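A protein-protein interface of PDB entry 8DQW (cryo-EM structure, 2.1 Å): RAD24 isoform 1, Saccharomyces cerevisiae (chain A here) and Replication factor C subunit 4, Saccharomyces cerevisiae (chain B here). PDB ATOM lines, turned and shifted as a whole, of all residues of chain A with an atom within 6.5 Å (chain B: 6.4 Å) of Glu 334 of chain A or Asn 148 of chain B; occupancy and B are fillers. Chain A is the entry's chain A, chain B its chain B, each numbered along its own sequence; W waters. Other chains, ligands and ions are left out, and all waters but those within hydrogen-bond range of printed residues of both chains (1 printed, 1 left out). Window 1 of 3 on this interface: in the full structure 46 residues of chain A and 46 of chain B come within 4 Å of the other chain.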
ATOM      1  N   GLU A 227     -20.901 -16.546 -15.454  1.00  0.00           N
ATOM      2  CA  GLU A 227     -20.740 -15.501 -14.458  1.00  0.00           C
ATOM      3  C   GLU A 227     -19.515 -15.774 -13.595  1.00  0.00           C
ATOM      4  O   GLU A 227     -19.168 -16.926 -13.317  1.00  0.00           O
ATOM      5  CB  GLU A 227     -21.985 -15.402 -13.576  1.00  0.00           C
ATOM      6  CG  GLU A 227     -23.162 -14.699 -14.236  1.00  0.00           C
ATOM      7  CD  GLU A 227     -23.651 -15.412 -15.481  1.00  0.00           C
ATOM      8  OE1 GLU A 227     -23.124 -15.127 -16.577  1.00  0.00           O
ATOM      9  OE2 GLU A 227     -24.563 -16.257 -15.365  1.00  0.00           O
ATOM     10  N   PRO A 229     -18.160 -15.691 -10.028  1.00  0.00           N
ATOM     11  CA  PRO A 229     -18.601 -15.546  -8.637  1.00  0.00           C
ATOM     12  C   PRO A 229     -17.779 -14.491  -7.912  1.00  0.00           C
ATOM     13  O   PRO A 229     -16.573 -14.356  -8.132  1.00  0.00           O
ATOM     14  CB  PRO A 229     -18.386 -16.942  -8.042  1.00  0.00           C
ATOM     15  CG  PRO A 229     -18.323 -17.860  -9.214  1.00  0.00           C
ATOM     16  CD  PRO A 229     -17.721 -17.065 -10.324  1.00  0.00           C
ATOM     17  N   THR A 332     -27.050 -32.234 -10.886  1.00  0.00           N
ATOM     18  CA  THR A 332     -26.166 -31.758 -11.938  1.00  0.00           C
ATOM     19  C   THR A 332     -25.577 -30.409 -11.537  1.00  0.00           C
ATOM     20  O   THR A 332     -25.847 -29.882 -10.454  1.00  0.00           O
ATOM     21  CB  THR A 332     -26.916 -31.647 -13.268  1.00  0.00           C
ATOM     22  OG1 THR A 332     -27.935 -30.645 -13.164  1.00  0.00           O
ATOM     23  CG2 THR A 332     -27.552 -32.979 -13.644  1.00  0.00           C
ATOM     24  N   ARG A 333     -24.763 -29.845 -12.426  1.00  0.00           N
ATOM     25  CA  ARG A 333     -24.196 -28.529 -12.171  1.00  0.00           C
ATOM     26  C   ARG A 333     -25.301 -27.481 -12.145  1.00  0.00           C
ATOM     27  O   ARG A 333     -26.270 -27.556 -12.906  1.00  0.00           O
ATOM     28  CB  ARG A 333     -23.149 -28.177 -13.234  1.00  0.00           C
ATOM     29  CG  ARG A 333     -23.697 -27.817 -14.617  1.00  0.00           C
ATOM     30  CD  ARG A 333     -22.667 -27.027 -15.413  1.00  0.00           C
ATOM     31  NE  ARG A 333     -23.122 -26.695 -16.759  1.00  0.00           N
ATOM     32  CZ  ARG A 333     -23.972 -25.718 -17.048  1.00  0.00           C
ATOM     33  NH1 ARG A 333     -24.509 -24.963 -16.103  1.00  0.00           N
ATOM     34  NH2 ARG A 333     -24.291 -25.492 -18.320  1.00  0.00           N
ATOM     35  N   GLU A 334     -25.159 -26.505 -11.253  1.00  0.00           N
ATOM     36  CA  GLU A 334     -26.128 -25.424 -11.178  1.00  0.00           C
ATOM     37  C   GLU A 334     -25.980 -24.506 -12.387  1.00  0.00           C
ATOM     38  O   GLU A 334     -24.883 -24.313 -12.918  1.00  0.00           O
ATOM     39  CB  GLU A 334     -25.945 -24.635  -9.880  1.00  0.00           C
ATOM     40  CG  GLU A 334     -26.936 -23.494  -9.682  1.00  0.00           C
ATOM     41  CD  GLU A 334     -26.520 -22.551  -8.572  1.00  0.00           C
ATOM     42  OE1 GLU A 334     -26.631 -22.940  -7.389  1.00  0.00           O
ATOM     43  OE2 GLU A 334     -26.084 -21.421  -8.880  1.00  0.00           O
ATOM     44  N   SER A 335     -27.104 -23.946 -12.827  1.00  0.00           N
ATOM     45  CA  SER A 335     -27.144 -23.050 -13.974  1.00  0.00           C
ATOM     46  C   SER A 335     -27.641 -21.682 -13.531  1.00  0.00           C
ATOM     47  O   SER A 335     -28.702 -21.576 -12.907  1.00  0.00           O
ATOM     48  CB  SER A 335     -28.047 -23.610 -15.076  1.00  0.00           C
ATOM     49  OG  SER A 335     -28.009 -22.792 -16.232  1.00  0.00           O
ATOM     50  N   THR A 336     -26.877 -20.643 -13.854  1.00  0.00           N
ATOM     51  CA  THR A 336     -27.291 -19.284 -13.542  1.00  0.00           C
ATOM     52  C   THR A 336     -28.427 -18.849 -14.463  1.00  0.00           C
ATOM     53  O   THR A 336     -28.547 -19.310 -15.602  1.00  0.00           O
ATOM     54  CB  THR A 336     -26.118 -18.314 -13.681  1.00  0.00           C
ATOM     55  OG1 THR A 336     -25.638 -18.329 -15.032  1.00  0.00           O
ATOM     56  CG2 THR A 336     -24.987 -18.694 -12.735  1.00  0.00           C
ATOM     57  N   GLU A 365     -29.315 -16.338  -2.815  1.00  0.00           N
ATOM     58  CA  GLU A 365     -28.213 -17.234  -2.484  1.00  0.00           C
ATOM     59  C   GLU A 365     -27.398 -17.594  -3.720  1.00  0.00           C
ATOM     60  O   GLU A 365     -26.174 -17.753  -3.636  1.00  0.00           O
ATOM     61  CB  GLU A 365     -28.751 -18.498  -1.812  1.00  0.00           C
ATOM     62  CG  GLU A 365     -27.897 -18.994  -0.658  1.00  0.00           C
ATOM     63  CD  GLU A 365     -26.593 -19.612  -1.121  1.00  0.00           C
ATOM     64  OE1 GLU A 365     -26.536 -20.090  -2.274  1.00  0.00           O
ATOM     65  OE2 GLU A 365     -25.625 -19.621  -0.333  1.00  0.00           O
ATOM     66  N   ASN A 366     -28.053 -17.723  -4.877  1.00  0.00           N
ATOM     67  CA  ASN A 366     -27.383 -18.183  -6.086  1.00  0.00           C
ATOM     68  C   ASN A 366     -27.138 -17.093  -7.120  1.00  0.00           C
ATOM     69  O   ASN A 366     -26.276 -17.276  -7.983  1.00  0.00           O
ATOM     70  CB  ASN A 366     -28.195 -19.308  -6.742  1.00  0.00           C
ATOM     71  CG  ASN A 366     -28.226 -20.568  -5.898  1.00  0.00           C
ATOM     72  OD1 ASN A 366     -27.185 -21.146  -5.590  1.00  0.00           O
ATOM     73  ND2 ASN A 366     -29.423 -20.995  -5.512  1.00  0.00           N
ATOM     74  N   SER A 367     -27.857 -15.975  -7.057  1.00  0.00           N
ATOM     75  CA  SER A 367     -27.716 -14.892  -8.026  1.00  0.00           C
ATOM     76  C   SER A 367     -27.402 -13.580  -7.324  1.00  0.00           C
ATOM     77  O   SER A 367     -27.851 -12.507  -7.739  1.00  0.00           O
ATOM     78  CB  SER A 367     -28.975 -14.758  -8.879  1.00  0.00           C
ATOM     79  OG  SER A 367     -30.124 -14.582  -8.069  1.00  0.00           O
ATOM     80  N   ASN A 368     -26.611 -13.645  -6.251  1.00  0.00           N
ATOM     81  CA  ASN A 368     -26.263 -12.433  -5.518  1.00  0.00           C
ATOM     82  C   ASN A 368     -25.532 -11.440  -6.411  1.00  0.00           C
ATOM     83  O   ASN A 368     -25.773 -10.230  -6.334  1.00  0.00           O
ATOM     84  CB  ASN A 368     -25.407 -12.781  -4.301  1.00  0.00           C
ATOM     85  CG  ASN A 368     -25.104 -11.573  -3.439  1.00  0.00           C
ATOM     86  OD1 ASN A 368     -26.007 -10.954  -2.877  1.00  0.00           O
ATOM     87  ND2 ASN A 368     -23.825 -11.228  -3.333  1.00  0.00           N
ATOM     88  N   CYS B 144     -15.220 -27.269  -1.053  1.00  0.00           N
ATOM     89  CA  CYS B 144     -15.664 -25.891  -0.906  1.00  0.00           C
ATOM     90  C   CYS B 144     -16.882 -25.856   0.002  1.00  0.00           C
ATOM     91  O   CYS B 144     -17.446 -26.891   0.364  1.00  0.00           O
ATOM     92  CB  CYS B 144     -15.985 -25.264  -2.266  1.00  0.00           C
ATOM     93  SG  CYS B 144     -17.276 -26.134  -3.187  1.00  0.00           S
ATOM     94  N   GLN B 146     -19.349 -23.298  -0.865  1.00  0.00           N
ATOM     95  CA  GLN B 146     -20.358 -22.842  -1.819  1.00  0.00           C
ATOM     96  C   GLN B 146     -19.987 -23.421  -3.181  1.00  0.00           C
ATOM     97  O   GLN B 146     -19.051 -22.944  -3.830  1.00  0.00           O
ATOM     98  CB  GLN B 146     -20.433 -21.319  -1.862  1.00  0.00           C
ATOM     99  CG  GLN B 146     -20.483 -20.661  -0.493  1.00  0.00           C
ATOM    100  CD  GLN B 146     -21.694 -21.087   0.315  1.00  0.00           C
ATOM    101  OE1 GLN B 146     -22.774 -21.307  -0.234  1.00  0.00           O
ATOM    102  NE2 GLN B 146     -21.519 -21.203   1.626  1.00  0.00           N
ATOM    103  N   SER B 147     -20.722 -24.449  -3.611  1.00  0.00           N
ATOM    104  CA  SER B 147     -20.425 -25.083  -4.890  1.00  0.00           C
ATOM    105  C   SER B 147     -20.605 -24.116  -6.052  1.00  0.00           C
ATOM    106  O   SER B 147     -20.003 -24.304  -7.114  1.00  0.00           O
ATOM    107  CB  SER B 147     -21.314 -26.311  -5.084  1.00  0.00           C
ATOM    108  OG  SER B 147     -20.843 -27.120  -6.145  1.00  0.00           O
ATOM    109  N   ASN B 148     -21.430 -23.082  -5.875  1.00  0.00           N
ATOM    110  CA  ASN B 148     -21.688 -22.132  -6.950  1.00  0.00           C
ATOM    111  C   ASN B 148     -20.517 -21.192  -7.204  1.00  0.00           C
ATOM    112  O   ASN B 148     -20.509 -20.512  -8.237  1.00  0.00           O
ATOM    113  CB  ASN B 148     -22.952 -21.323  -6.637  1.00  0.00           C
ATOM    114  CG  ASN B 148     -22.652 -19.990  -5.980  1.00  0.00           C
ATOM    115  OD1 ASN B 148     -21.814 -19.898  -5.082  1.00  0.00           O
ATOM    116  ND2 ASN B 148     -23.339 -18.945  -6.426  1.00  0.00           N
ATOM    117  N   LYS B 149     -19.535 -21.137  -6.306  1.00  0.00           N
ATOM    118  CA  LYS B 149     -18.380 -20.269  -6.492  1.00  0.00           C
ATOM    119  C   LYS B 149     -17.328 -20.879  -7.412  1.00  0.00           C
ATOM    120  O   LYS B 149     -16.333 -20.212  -7.715  1.00  0.00           O
ATOM    121  CB  LYS B 149     -17.754 -19.928  -5.134  1.00  0.00           C
ATOM    122  CG  LYS B 149     -18.126 -18.537  -4.633  1.00  0.00           C
ATOM    123  CD  LYS B 149     -17.412 -18.184  -3.334  1.00  0.00           C
ATOM    124  CE  LYS B 149     -15.995 -17.676  -3.576  1.00  0.00           C
ATOM    125  NZ  LYS B 149     -15.939 -16.505  -4.493  1.00  0.00           N
ATOM    126  N   ILE B 150     -17.520 -22.117  -7.855  1.00  0.00           N
ATOM    127  CA  ILE B 150     -16.685 -22.720  -8.887  1.00  0.00           C
ATOM    128  C   ILE B 150     -17.345 -22.465 -10.236  1.00  0.00           C
ATOM    129  O   ILE B 150     -18.549 -22.693 -10.399  1.00  0.00           O
ATOM    130  CB  ILE B 150     -16.495 -24.225  -8.634  1.00  0.00           C
ATOM    131  CG1 ILE B 150     -15.931 -24.457  -7.225  1.00  0.00           C
ATOM    132  CG2 ILE B 150     -15.586 -24.837  -9.693  1.00  0.00           C
ATOM    133  CD1 ILE B 150     -15.733 -25.913  -6.868  1.00  0.00           C
ATOM    134  N   ILE B 151     -16.562 -21.980 -11.205  1.00  0.00           N
ATOM    135  CA  ILE B 151     -17.141 -21.570 -12.478  1.00  0.00           C
ATOM    136  C   ILE B 151     -17.811 -22.761 -13.161  1.00  0.00           C
ATOM    137  O   ILE B 151     -17.387 -23.914 -13.018  1.00  0.00           O
ATOM    138  CB  ILE B 151     -16.080 -20.936 -13.395  1.00  0.00           C
ATOM    139  CG1 ILE B 151     -14.940 -21.918 -13.677  1.00  0.00           C
ATOM    140  CG2 ILE B 151     -15.539 -19.658 -12.771  1.00  0.00           C
ATOM    141  CD1 ILE B 151     -14.032 -21.482 -14.806  1.00  0.00           C
ATOM    142  N   GLU B 152     -18.867 -22.468 -13.918  1.00  0.00           N
ATOM    143  CA  GLU B 152     -19.668 -23.531 -14.521  1.00  0.00           C
ATOM    144  C   GLU B 152     -18.867 -24.465 -15.419  1.00  0.00           C
ATOM    145  O   GLU B 152     -19.121 -25.681 -15.374  1.00  0.00           O
ATOM    146  CB  GLU B 152     -20.838 -22.915 -15.298  1.00  0.00           C
ATOM    147  CG  GLU B 152     -22.172 -23.032 -14.576  1.00  0.00           C
ATOM    148  CD  GLU B 152     -23.079 -21.836 -14.802  1.00  0.00           C
ATOM    149  OE1 GLU B 152     -22.819 -21.051 -15.737  1.00  0.00           O
ATOM    150  OE2 GLU B 152     -24.060 -21.687 -14.044  1.00  0.00           O
ATOM    151  N   GLN B 155     -17.534 -27.036 -13.143  1.00  0.00           N
ATOM    152  CA  GLN B 155     -18.584 -27.892 -12.596  1.00  0.00           C
ATOM    153  C   GLN B 155     -19.042 -28.920 -13.620  1.00  0.00           C
ATOM    154  O   GLN B 155     -19.413 -30.044 -13.262  1.00  0.00           O
ATOM    155  CB  GLN B 155     -19.782 -27.059 -12.137  1.00  0.00           C
ATOM    156  CG  GLN B 155     -19.460 -25.896 -11.213  1.00  0.00           C
ATOM    157  CD  GLN B 155     -20.709 -25.188 -10.705  1.00  0.00           C
ATOM    158  OE1 GLN B 155     -20.736 -23.965 -10.586  1.00  0.00           O
ATOM    159  NE2 GLN B 155     -21.746 -25.958 -10.387  1.00  0.00           N
ATOM    160  N   ILE B 160     -21.069 -33.890  -8.416  1.00  0.00           N
ATOM    161  CA  ILE B 160     -21.363 -33.031  -7.275  1.00  0.00           C
ATOM    162  C   ILE B 160     -21.717 -33.900  -6.080  1.00  0.00           C
ATOM    163  O   ILE B 160     -22.390 -34.929  -6.218  1.00  0.00           O
ATOM    164  CB  ILE B 160     -22.503 -32.044  -7.600  1.00  0.00           C
ATOM    165  CG1 ILE B 160     -22.457 -31.605  -9.071  1.00  0.00           C
ATOM    166  CG2 ILE B 160     -22.443 -30.844  -6.666  1.00  0.00           C
ATOM    167  CD1 ILE B 160     -21.231 -30.792  -9.436  1.00  0.00           C
ATOM    168  N   ARG B 162     -23.011 -33.027  -2.104  1.00  0.00           N
ATOM    169  CA  ARG B 162     -23.383 -32.043  -1.099  1.00  0.00           C
ATOM    170  C   ARG B 162     -23.492 -32.732   0.256  1.00  0.00           C
ATOM    171  O   ARG B 162     -24.264 -33.683   0.411  1.00  0.00           O
ATOM    172  CB  ARG B 162     -24.703 -31.368  -1.469  1.00  0.00           C
ATOM    173  CG  ARG B 162     -24.895 -31.176  -2.968  1.00  0.00           C
ATOM    174  CD  ARG B 162     -25.778 -29.977  -3.275  1.00  0.00           C
ATOM    175  NE  ARG B 162     -25.817 -29.677  -4.702  1.00  0.00           N
ATOM    176  CZ  ARG B 162     -25.077 -28.753  -5.303  1.00  0.00           C
ATOM    177  NH1 ARG B 162     -24.207 -28.015  -4.633  1.00  0.00           N
ATOM    178  NH2 ARG B 162     -25.212 -28.567  -6.613  1.00  0.00           N
HETATM  179  O   HOH W   1     -20.026 -19.726 -13.677  1.00  0.00           O
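The side-chain amide oxygen of Gln 146 of chain B sits close to the side-chain carboxylate of Glu 365 of chain A, at 3.3 Å. NH1 of Arg 333 of chain A lies within salt-bridge range of OE2 of Glu 152 of chain B. OE2 of Glu 152 of chain B lies within hydrogen-bond range of N of Thr 336 of chain A, 3.0 Å away. The side-chain carboxylate (OE2) of Glu 152 of chain B lies close to the backbone carbonyl oxygen (O) of Glu 334 of chain A, at 3.0 Å.
The side-chain sulfur of Cys 144 of chain B is in hydrogen-bond range of the backbone carbonyl oxygen of Gln 146 of chain B. O of Ile 150 of chain B sits close to OE1 of Gln 155 of chain B (2.5 Å). OD1 of Asn 366 of chain A lies close to OE1 of Glu 334 of chain A.
Hydrophobic or aromatic side chains of chain A within 4 Å of the printed part of chain B: Pro 229. Among the printed residues, 11 pairs touch across the chains. Among the printed residues, Asp or Glu carboxylates within 4 Å of a Lys or Arg side-chain nitrogen of the other chain: Arg 333 of chain A with Glu 152 of chain B.
Water W1 bridges the backbone carbonyl oxygen of Glu 227 of chain A and the backbone NH of Glu 152 of chain B.
Asn 148 of chain B touches just these residues of chain A: Pro 229, Glu 334 and Asn 366. Printed residues of chain B within 4 Å of Ser 335 of chain A: Glu 152. Printed residues of chain A within 4 Å of Glu 152 of chain B: Arg 333 (3.4 Å), Glu 334 (3.0 Å), Ser 335 (3.4 Å) and Thr 336 (3.0 Å). Printed residues of chain B within 4 Å of Thr 336 of chain A: Glu 152 (3.0 Å). Thr 332 of chain A touches none of the printed residues of chain B. The nearest residue of chain A that does not touch Asn 148 of chain B is Glu 365 of chain A (4.2 Å).
Asn 148 of chain B touches Pro 229 of chain A (O to CG, 3.6 Å). Lys 149 of chain B touches Pro 229 of chain A. CB of Arg 333 of chain A touches CB of Gln 155 of chain B, 3.7 Å away. OE2 of Glu 334 of chain A touches CB of Asn 148 of chain B, 3.9 Å away. NE2 of Gln 155 of chain B touches N of Glu 334 of chain A (3.6 Å). Glu 152 of chain B touches Ser 335 of chain A. ND2 of Asn 148 of chain B touches O of Asn 366 of chain A (3.7 Å).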
